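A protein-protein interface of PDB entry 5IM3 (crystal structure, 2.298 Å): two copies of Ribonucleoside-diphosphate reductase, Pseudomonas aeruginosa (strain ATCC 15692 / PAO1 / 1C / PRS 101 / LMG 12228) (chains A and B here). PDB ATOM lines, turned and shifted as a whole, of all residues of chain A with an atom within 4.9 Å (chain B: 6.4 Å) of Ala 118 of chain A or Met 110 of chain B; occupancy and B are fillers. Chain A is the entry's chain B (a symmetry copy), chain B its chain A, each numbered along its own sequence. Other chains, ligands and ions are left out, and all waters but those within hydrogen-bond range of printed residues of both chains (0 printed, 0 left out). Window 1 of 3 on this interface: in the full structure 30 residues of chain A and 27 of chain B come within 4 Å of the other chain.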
ATOM      1  N   LEU A 109     -21.618  11.258  25.853  1.00  0.00           N
ATOM      2  CA  LEU A 109     -21.219  10.295  24.832  1.00  0.00           C
ATOM      3  C   LEU A 109     -21.736  10.709  23.461  1.00  0.00           C
ATOM      4  O   LEU A 109     -21.031  10.578  22.454  1.00  0.00           O
ATOM      5  CB  LEU A 109     -21.742   8.903  25.193  1.00  0.00           C
ATOM      6  CG  LEU A 109     -21.108   8.206  26.396  1.00  0.00           C
ATOM      7  CD1 LEU A 109     -22.021   7.106  26.902  1.00  0.00           C
ATOM      8  CD2 LEU A 109     -19.744   7.640  26.030  1.00  0.00           C
ATOM      9  N   MET A 110     -22.968  11.215  23.408  1.00  0.00           N
ATOM     10  CA  MET A 110     -23.584  11.557  22.132  1.00  0.00           C
ATOM     11  C   MET A 110     -22.898  12.754  21.480  1.00  0.00           C
ATOM     12  O   MET A 110     -22.662  12.752  20.267  1.00  0.00           O
ATOM     13  CB  MET A 110     -25.074  11.824  22.343  1.00  0.00           C
ATOM     14  CG  MET A 110     -25.864  10.575  22.711  1.00  0.00           C
ATOM     15  SD  MET A 110     -27.618  10.910  22.953  1.00  0.00           S
ATOM     16  CE  MET A 110     -28.262   9.262  23.221  1.00  0.00           C
ATOM     17  N   ARG A 111     -22.570  13.788  22.260  1.00  0.00           N
ATOM     18  CA  ARG A 111     -21.902  14.950  21.677  1.00  0.00           C
ATOM     19  C   ARG A 111     -20.500  14.605  21.188  1.00  0.00           C
ATOM     20  O   ARG A 111     -20.037  15.172  20.192  1.00  0.00           O
ATOM     21  CB  ARG A 111     -21.832  16.094  22.688  1.00  0.00           C
ATOM     22  CG  ARG A 111     -23.153  16.798  22.940  1.00  0.00           C
ATOM     23  CD  ARG A 111     -23.003  18.301  22.789  1.00  0.00           C
ATOM     24  NE  ARG A 111     -24.092  19.029  23.436  1.00  0.00           N
ATOM     25  CZ  ARG A 111     -24.105  19.374  24.721  1.00  0.00           C
ATOM     26  NH1 ARG A 111     -23.089  19.058  25.516  1.00  0.00           N
ATOM     27  NH2 ARG A 111     -25.143  20.036  25.215  1.00  0.00           N
ATOM     28  N   GLU A 114     -19.599   9.283  19.966  1.00  0.00           N
ATOM     29  CA  GLU A 114     -19.448   7.863  20.283  1.00  0.00           C
ATOM     30  C   GLU A 114     -20.792   7.162  20.076  1.00  0.00           C
ATOM     31  O   GLU A 114     -21.482   6.758  21.014  1.00  0.00           O
ATOM     32  CB  GLU A 114     -18.935   7.689  21.706  1.00  0.00           C
ATOM     33  CG  GLU A 114     -17.571   8.321  21.967  1.00  0.00           C
ATOM     34  CD  GLU A 114     -16.448   7.621  21.224  1.00  0.00           C
ATOM     35  OE1 GLU A 114     -16.668   6.498  20.725  1.00  0.00           O
ATOM     36  OE2 GLU A 114     -15.345   8.196  21.136  1.00  0.00           O
ATOM     37  N   GLN A 115     -21.156   7.017  18.800  1.00  0.00           N
ATOM     38  CA  GLN A 115     -22.475   6.491  18.460  1.00  0.00           C
ATOM     39  C   GLN A 115     -22.629   5.037  18.890  1.00  0.00           C
ATOM     40  O   GLN A 115     -23.671   4.652  19.432  1.00  0.00           O
ATOM     41  CB  GLN A 115     -22.717   6.639  16.958  1.00  0.00           C
ATOM     42  CG  GLN A 115     -24.054   6.095  16.480  1.00  0.00           C
ATOM     43  CD  GLN A 115     -23.945   4.710  15.862  1.00  0.00           C
ATOM     44  OE1 GLN A 115     -22.854   4.250  15.517  1.00  0.00           O
ATOM     45  NE2 GLN A 115     -25.081   4.041  15.716  1.00  0.00           N
ATOM     46  N   LYS A 116     -21.610   4.212  18.646  1.00  0.00           N
ATOM     47  CA  LYS A 116     -21.666   2.815  19.065  1.00  0.00           C
ATOM     48  C   LYS A 116     -21.811   2.704  20.578  1.00  0.00           C
ATOM     49  O   LYS A 116     -22.700   2.006  21.080  1.00  0.00           O
ATOM     50  CB  LYS A 116     -20.413   2.077  18.595  1.00  0.00           C
ATOM     51  CG  LYS A 116     -20.616   1.228  17.358  1.00  0.00           C
ATOM     52  CD  LYS A 116     -21.485   0.019  17.657  1.00  0.00           C
ATOM     53  CE  LYS A 116     -21.361  -1.031  16.567  1.00  0.00           C
ATOM     54  NZ  LYS A 116     -21.655  -0.471  15.217  1.00  0.00           N
ATOM     55  N   VAL A 117     -20.944   3.390  21.321  1.00  0.00           N
ATOM     56  CA  VAL A 117     -20.965   3.286  22.775  1.00  0.00           C
ATOM     57  C   VAL A 117     -22.240   3.900  23.336  1.00  0.00           C
ATOM     58  O   VAL A 117     -22.827   3.378  24.291  1.00  0.00           O
ATOM     59  CB  VAL A 117     -19.705   3.948  23.366  1.00  0.00           C
ATOM     60  CG1 VAL A 117     -19.733   3.911  24.886  1.00  0.00           C
ATOM     61  CG2 VAL A 117     -18.459   3.255  22.843  1.00  0.00           C
ATOM     62  N   ALA A 118     -22.690   5.014  22.755  1.00  0.00           N
ATOM     63  CA  ALA A 118     -23.887   5.680  23.259  1.00  0.00           C
ATOM     64  C   ALA A 118     -25.112   4.789  23.107  1.00  0.00           C
ATOM     65  O   ALA A 118     -25.895   4.625  24.050  1.00  0.00           O
ATOM     66  CB  ALA A 118     -24.097   7.011  22.534  1.00  0.00           C
ATOM     67  N   ARG A 119     -25.298   4.201  21.923  1.00  0.00           N
ATOM     68  CA  ARG A 119     -26.472   3.363  21.718  1.00  0.00           C
ATOM     69  C   ARG A 119     -26.418   2.131  22.611  1.00  0.00           C
ATOM     70  O   ARG A 119     -27.443   1.712  23.158  1.00  0.00           O
ATOM     71  CB  ARG A 119     -26.603   2.976  20.241  1.00  0.00           C
ATOM     72  CG  ARG A 119     -25.627   1.912  19.756  1.00  0.00           C
ATOM     73  CD  ARG A 119     -25.702   1.723  18.244  1.00  0.00           C
ATOM     74  NE  ARG A 119     -27.081   1.727  17.772  1.00  0.00           N
ATOM     75  CZ  ARG A 119     -27.898   0.684  17.848  1.00  0.00           C
ATOM     76  NH1 ARG A 119     -27.474  -0.457  18.374  1.00  0.00           N
ATOM     77  NH2 ARG A 119     -29.141   0.785  17.399  1.00  0.00           N
ATOM     78  N   ASP A 120     -25.223   1.561  22.806  1.00  0.00           N
ATOM     79  CA  ASP A 120     -25.090   0.418  23.704  1.00  0.00           C
ATOM     80  C   ASP A 120     -25.331   0.818  25.154  1.00  0.00           C
ATOM     81  O   ASP A 120     -25.866   0.025  25.934  1.00  0.00           O
ATOM     82  CB  ASP A 120     -23.705  -0.217  23.559  1.00  0.00           C
ATOM     83  CG  ASP A 120     -23.540  -0.977  22.255  1.00  0.00           C
ATOM     84  OD1 ASP A 120     -24.549  -1.200  21.554  1.00  0.00           O
ATOM     85  OD2 ASP A 120     -22.396  -1.363  21.937  1.00  0.00           O
ATOM     86  N   TYR A 121     -24.934   2.034  25.532  1.00  0.00           N
ATOM     87  CA  TYR A 121     -25.241   2.530  26.869  1.00  0.00           C
ATOM     88  C   TYR A 121     -26.745   2.659  27.069  1.00  0.00           C
ATOM     89  O   TYR A 121     -27.274   2.310  28.131  1.00  0.00           O
ATOM     90  CB  TYR A 121     -24.556   3.881  27.093  1.00  0.00           C
ATOM     91  CG  TYR A 121     -24.455   4.283  28.548  1.00  0.00           C
ATOM     92  CD1 TYR A 121     -25.534   4.849  29.214  1.00  0.00           C
ATOM     93  CD2 TYR A 121     -23.274   4.099  29.254  1.00  0.00           C
ATOM     94  CE1 TYR A 121     -25.439   5.218  30.545  1.00  0.00           C
ATOM     95  CE2 TYR A 121     -23.171   4.461  30.582  1.00  0.00           C
ATOM     96  CZ  TYR A 121     -24.252   5.018  31.224  1.00  0.00           C
ATOM     97  OH  TYR A 121     -24.138   5.371  32.548  1.00  0.00           O
ATOM     98  N   VAL A 122     -27.450   3.159  26.052  1.00  0.00           N
ATOM     99  CA  VAL A 122     -28.901   3.304  26.137  1.00  0.00           C
ATOM    100  C   VAL A 122     -29.564   1.939  26.260  1.00  0.00           C
ATOM    101  O   VAL A 122     -30.388   1.711  27.152  1.00  0.00           O
ATOM    102  CB  VAL A 122     -29.430   4.077  24.916  1.00  0.00           C
ATOM    103  CG1 VAL A 122     -30.953   4.034  24.866  1.00  0.00           C
ATOM    104  CG2 VAL A 122     -28.942   5.505  24.961  1.00  0.00           C
ATOM    105  N   VAL B 105     -27.574   8.203  10.855  1.00  0.00           N
ATOM    106  CA  VAL B 105     -28.694   8.998  11.350  1.00  0.00           C
ATOM    107  C   VAL B 105     -28.574   9.191  12.856  1.00  0.00           C
ATOM    108  O   VAL B 105     -28.721  10.308  13.368  1.00  0.00           O
ATOM    109  CB  VAL B 105     -30.033   8.340  10.967  1.00  0.00           C
ATOM    110  CG1 VAL B 105     -31.190   8.954  11.757  1.00  0.00           C
ATOM    111  CG2 VAL B 105     -30.281   8.483   9.469  1.00  0.00           C
ATOM    112  N   GLU B 106     -28.314   8.105  13.588  1.00  0.00           N
ATOM    113  CA  GLU B 106     -28.099   8.222  15.026  1.00  0.00           C
ATOM    114  C   GLU B 106     -26.941   9.161  15.324  1.00  0.00           C
ATOM    115  O   GLU B 106     -27.006   9.962  16.263  1.00  0.00           O
ATOM    116  CB  GLU B 106     -27.833   6.848  15.642  1.00  0.00           C
ATOM    117  CG  GLU B 106     -29.033   5.909  15.651  1.00  0.00           C
ATOM    118  CD  GLU B 106     -28.718   4.555  16.274  1.00  0.00           C
ATOM    119  OE1 GLU B 106     -27.545   4.321  16.647  1.00  0.00           O
ATOM    120  OE2 GLU B 106     -29.645   3.721  16.393  1.00  0.00           O
ATOM    121  N   LEU B 107     -25.872   9.081  14.530  1.00  0.00           N
ATOM    122  CA  LEU B 107     -24.713   9.936  14.757  1.00  0.00           C
ATOM    123  C   LEU B 107     -25.093  11.408  14.653  1.00  0.00           C
ATOM    124  O   LEU B 107     -24.724  12.218  15.510  1.00  0.00           O
ATOM    125  CB  LEU B 107     -23.606   9.585  13.761  1.00  0.00           C
ATOM    126  CG  LEU B 107     -22.324  10.423  13.842  1.00  0.00           C
ATOM    127  CD1 LEU B 107     -21.670  10.296  15.214  1.00  0.00           C
ATOM    128  CD2 LEU B 107     -21.347  10.023  12.746  1.00  0.00           C
ATOM    129  N   ALA B 108     -25.844  11.771  13.610  1.00  0.00           N
ATOM    130  CA  ALA B 108     -26.219  13.168  13.415  1.00  0.00           C
ATOM    131  C   ALA B 108     -27.096  13.666  14.559  1.00  0.00           C
ATOM    132  O   ALA B 108     -26.881  14.761  15.090  1.00  0.00           O
ATOM    133  CB  ALA B 108     -26.934  13.335  12.074  1.00  0.00           C
ATOM    134  N   LEU B 109     -28.100  12.874  14.947  1.00  0.00           N
ATOM    135  CA  LEU B 109     -28.933  13.242  16.089  1.00  0.00           C
ATOM    136  C   LEU B 109     -28.092  13.414  17.348  1.00  0.00           C
ATOM    137  O   LEU B 109     -28.306  14.353  18.125  1.00  0.00           O
ATOM    138  CB  LEU B 109     -30.012  12.183  16.317  1.00  0.00           C
ATOM    139  CG  LEU B 109     -31.227  12.221  15.388  1.00  0.00           C
ATOM    140  CD1 LEU B 109     -31.975  10.891  15.429  1.00  0.00           C
ATOM    141  CD2 LEU B 109     -32.151  13.371  15.768  1.00  0.00           C
ATOM    142  N   MET B 110     -27.122  12.521  17.558  1.00  0.00           N
ATOM    143  CA  MET B 110     -26.343  12.539  18.791  1.00  0.00           C
ATOM    144  C   MET B 110     -25.387  13.726  18.837  1.00  0.00           C
ATOM    145  O   MET B 110     -25.269  14.389  19.873  1.00  0.00           O
ATOM    146  CB  MET B 110     -25.574  11.230  18.936  1.00  0.00           C
ATOM    147  CG  MET B 110     -26.451  10.037  19.256  1.00  0.00           C
ATOM    148  SD  MET B 110     -25.490   8.521  19.347  1.00  0.00           S
ATOM    149  CE  MET B 110     -26.773   7.312  19.672  1.00  0.00           C
ATOM    150  N   ARG B 111     -24.679  14.003  17.737  1.00  0.00           N
ATOM    151  CA  ARG B 111     -23.749  15.126  17.736  1.00  0.00           C
ATOM    152  C   ARG B 111     -24.469  16.457  17.892  1.00  0.00           C
ATOM    153  O   ARG B 111     -23.858  17.425  18.353  1.00  0.00           O
ATOM    154  CB  ARG B 111     -22.911  15.135  16.455  1.00  0.00           C
ATOM    155  CG  ARG B 111     -21.956  13.958  16.329  1.00  0.00           C
ATOM    156  CD  ARG B 111     -20.912  14.196  15.250  1.00  0.00           C
ATOM    157  NE  ARG B 111     -19.741  14.904  15.772  1.00  0.00           N
ATOM    158  CZ  ARG B 111     -18.577  14.331  16.074  1.00  0.00           C
ATOM    159  NH1 ARG B 111     -18.393  13.026  15.904  1.00  0.00           N
ATOM    160  NH2 ARG B 111     -17.579  15.071  16.543  1.00  0.00           N
ATOM    161  N   ALA B 112     -25.746  16.523  17.518  1.00  0.00           N
ATOM    162  CA  ALA B 112     -26.564  17.709  17.720  1.00  0.00           C
ATOM    163  C   ALA B 112     -27.101  17.825  19.141  1.00  0.00           C
ATOM    164  O   ALA B 112     -27.874  18.746  19.419  1.00  0.00           O
ATOM    165  CB  ALA B 112     -27.734  17.711  16.733  1.00  0.00           C
ATOM    166  N   GLY B 113     -26.717  16.922  20.039  1.00  0.00           N
ATOM    167  CA  GLY B 113     -27.189  16.982  21.407  1.00  0.00           C
ATOM    168  C   GLY B 113     -28.651  16.646  21.598  1.00  0.00           C
ATOM    169  O   GLY B 113     -29.226  17.009  22.626  1.00  0.00           O
ATOM    170  N   GLU B 114     -29.274  15.960  20.636  1.00  0.00           N
ATOM    171  CA  GLU B 114     -30.680  15.566  20.748  1.00  0.00           C
ATOM    172  C   GLU B 114     -30.764  14.261  21.542  1.00  0.00           C
ATOM    173  O   GLU B 114     -30.995  13.174  21.011  1.00  0.00           O
ATOM    174  CB  GLU B 114     -31.308  15.419  19.369  1.00  0.00           C
ATOM    175  CG  GLU B 114     -31.271  16.679  18.518  1.00  0.00           C
ATOM    176  CD  GLU B 114     -32.297  17.714  18.944  1.00  0.00           C
ATOM    177  OE1 GLU B 114     -33.110  17.414  19.844  1.00  0.00           O
ATOM    178  OE2 GLU B 114     -32.293  18.828  18.372  1.00  0.00           O
ATOM    179  N   GLN B 115     -30.572  14.392  22.855  1.00  0.00           N
ATOM    180  CA  GLN B 115     -30.442  13.211  23.702  1.00  0.00           C
ATOM    181  C   GLN B 115     -31.735  12.406  23.749  1.00  0.00           C
ATOM    182  O   GLN B 115     -31.705  11.175  23.648  1.00  0.00           O
ATOM    183  CB  GLN B 115     -30.016  13.620  25.112  1.00  0.00           C
ATOM    184  CG  GLN B 115     -29.580  12.455  25.994  1.00  0.00           C
ATOM    185  CD  GLN B 115     -30.600  12.103  27.060  1.00  0.00           C
ATOM    186  OE1 GLN B 115     -31.363  12.956  27.511  1.00  0.00           O
ATOM    187  NE2 GLN B 115     -30.616  10.838  27.469  1.00  0.00           N
ATOM    188  N   ALA B 118     -32.557  11.040  20.112  1.00  0.00           N
ATOM    189  CA  ALA B 118     -31.586  10.032  19.702  1.00  0.00           C
ATOM    190  C   ALA B 118     -31.824   8.714  20.429  1.00  0.00           C
ATOM    191  O   ALA B 118     -31.819   7.643  19.811  1.00  0.00           O
ATOM    192  CB  ALA B 118     -30.165  10.534  19.952  1.00  0.00           C
ATOM    193  N   ARG B 119     -32.041   8.771  21.745  1.00  0.00           N
ATOM    194  CA  ARG B 119     -32.177   7.539  22.515  1.00  0.00           C
ATOM    195  C   ARG B 119     -33.472   6.814  22.171  1.00  0.00           C
ATOM    196  O   ARG B 119     -33.509   5.579  22.144  1.00  0.00           O
ATOM    197  CB  ARG B 119     -32.101   7.834  24.014  1.00  0.00           C
ATOM    198  CG  ARG B 119     -33.407   8.260  24.656  1.00  0.00           C
ATOM    199  CD  ARG B 119     -33.182   8.744  26.083  1.00  0.00           C
ATOM    200  NE  ARG B 119     -32.367   7.820  26.870  1.00  0.00           N
ATOM    201  CZ  ARG B 119     -32.838   6.750  27.508  1.00  0.00           C
ATOM    202  NH1 ARG B 119     -34.130   6.450  27.456  1.00  0.00           N
ATOM    203  NH2 ARG B 119     -32.011   5.972  28.197  1.00  0.00           N
ATOM    204  N   VAL B 122     -32.771   5.073  18.957  1.00  0.00           N
ATOM    205  CA  VAL B 122     -32.040   3.835  19.220  1.00  0.00           C
ATOM    206  C   VAL B 122     -32.988   2.761  19.738  1.00  0.00           C
ATOM    207  O   VAL B 122     -33.017   1.633  19.230  1.00  0.00           O
ATOM    208  CB  VAL B 122     -30.891   4.095  20.214  1.00  0.00           C
ATOM    209  CG1 VAL B 122     -30.359   2.783  20.792  1.00  0.00           C
ATOM    210  CG2 VAL B 122     -29.766   4.866  19.543  1.00  0.00           C
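Hydrophobic or aromatic side chains of chain B that line the printed part of chain A: Met 110, Ala 118 and Val 122.
Hydrophobic or aromatic side chains of chain A that line the printed part of chain B: Met 110, Ala 118 and Val 122.
Among the printed residues, 11 pairs touch across the chains.
The side-chain amide nitrogen (NE2) of Gln 115 of chain A sits at hydrogen-bond distance from the side-chain carboxylate (OE1) of Glu 106 of chain B (2.6 Å).
NE of Arg 119 of chain A is in salt-bridge range of OE1 of Glu 106 of chain B, 2.9 Å away.
The backbone NH (N) of Arg 111 of chain B sits at hydrogen-bond distance from the backbone carbonyl oxygen (O) of Met 110 of chain A (3.5 Å).
The backbone carbonyl oxygen (O) of Met 110 of chain A sits close to the backbone carbonyl oxygen (O) of Met 110 of chain B (3.1 Å).
Printed residues of chain B within 4 Å of Arg 111 of chain A: Met 110.
Of the printed residues of chain B, Gln 115 of chain A touches Glu 106 (2.6 Å) and Met 110 (3.7 Å).
Printed residues of chain B within 4 Å of Ala 118 of chain A: Met 110 (3.8 Å).
Printed residues of chain B within 4 Å of Arg 119 of chain A: Glu 106 and Val 122.
Tyr 121 of chain A touches none of the printed residues of chain B.
Of chain A, only Met 110 (3.1 Å), Arg 111 (3.7 Å), Gln 115 (3.7 Å) and Ala 118 (3.8 Å) come within 4 Å of Met 110 of chain B.
Of the printed residues of chain A, Arg 111 of chain B touches Met 110 (3.5 Å).
Printed residues of chain A within 4 Å of Gln 115 of chain B: Met 110 (3.7 Å).
The nearest residue of chain B that does not touch Ala 118 of chain A is Val 122 of chain B (5.8 Å).
The nearest residue of chain A that does not touch Met 110 of chain B is Arg 119 of chain A (4.1 Å).
The nearest printed residue of chain B that does not touch Arg 111 of chain A is Gly 113 of chain B (4.2 Å).
Met 110 of chain B touches its own counterpart, Met 110 of chain A.
Met 110 of chain A touches Gln 115 of chain B, and with the chains exchanged Gln 115 of chain A touches Met 110 of chain B.
Met 110 of chain A touches Ala 118 of chain B, and with the chains exchanged Ala 118 of chain A touches Met 110 of chain B.
Arg 119 of chain A touches Val 122 of chain B, and with the chains exchanged Val 122 of chain A touches Arg 119 of chain B.
Positions printed for both chains: 109, 110, 111, 114, 115, 118, 119 and 122.
Among the printed residues, pairs that only touch across the chains: Met 110 of chain A with Gln 115 of chain B (3.7 Å), Met 110 of chain A with Ala 118 of chain B (3.95 Å), Arg 111 of chain A with Met 110 of chain B (3.7 Å), Gln 115 of chain A with Met 110 of chain B (3.7 Å), Ala 118 of chain A with Met 110 of chain B (3.8 Å), Arg 119 of chain A with Val 122 of chain B (3.8 Å) and Val 122 of chain A with Arg 119 of chain B (3.996 Å).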
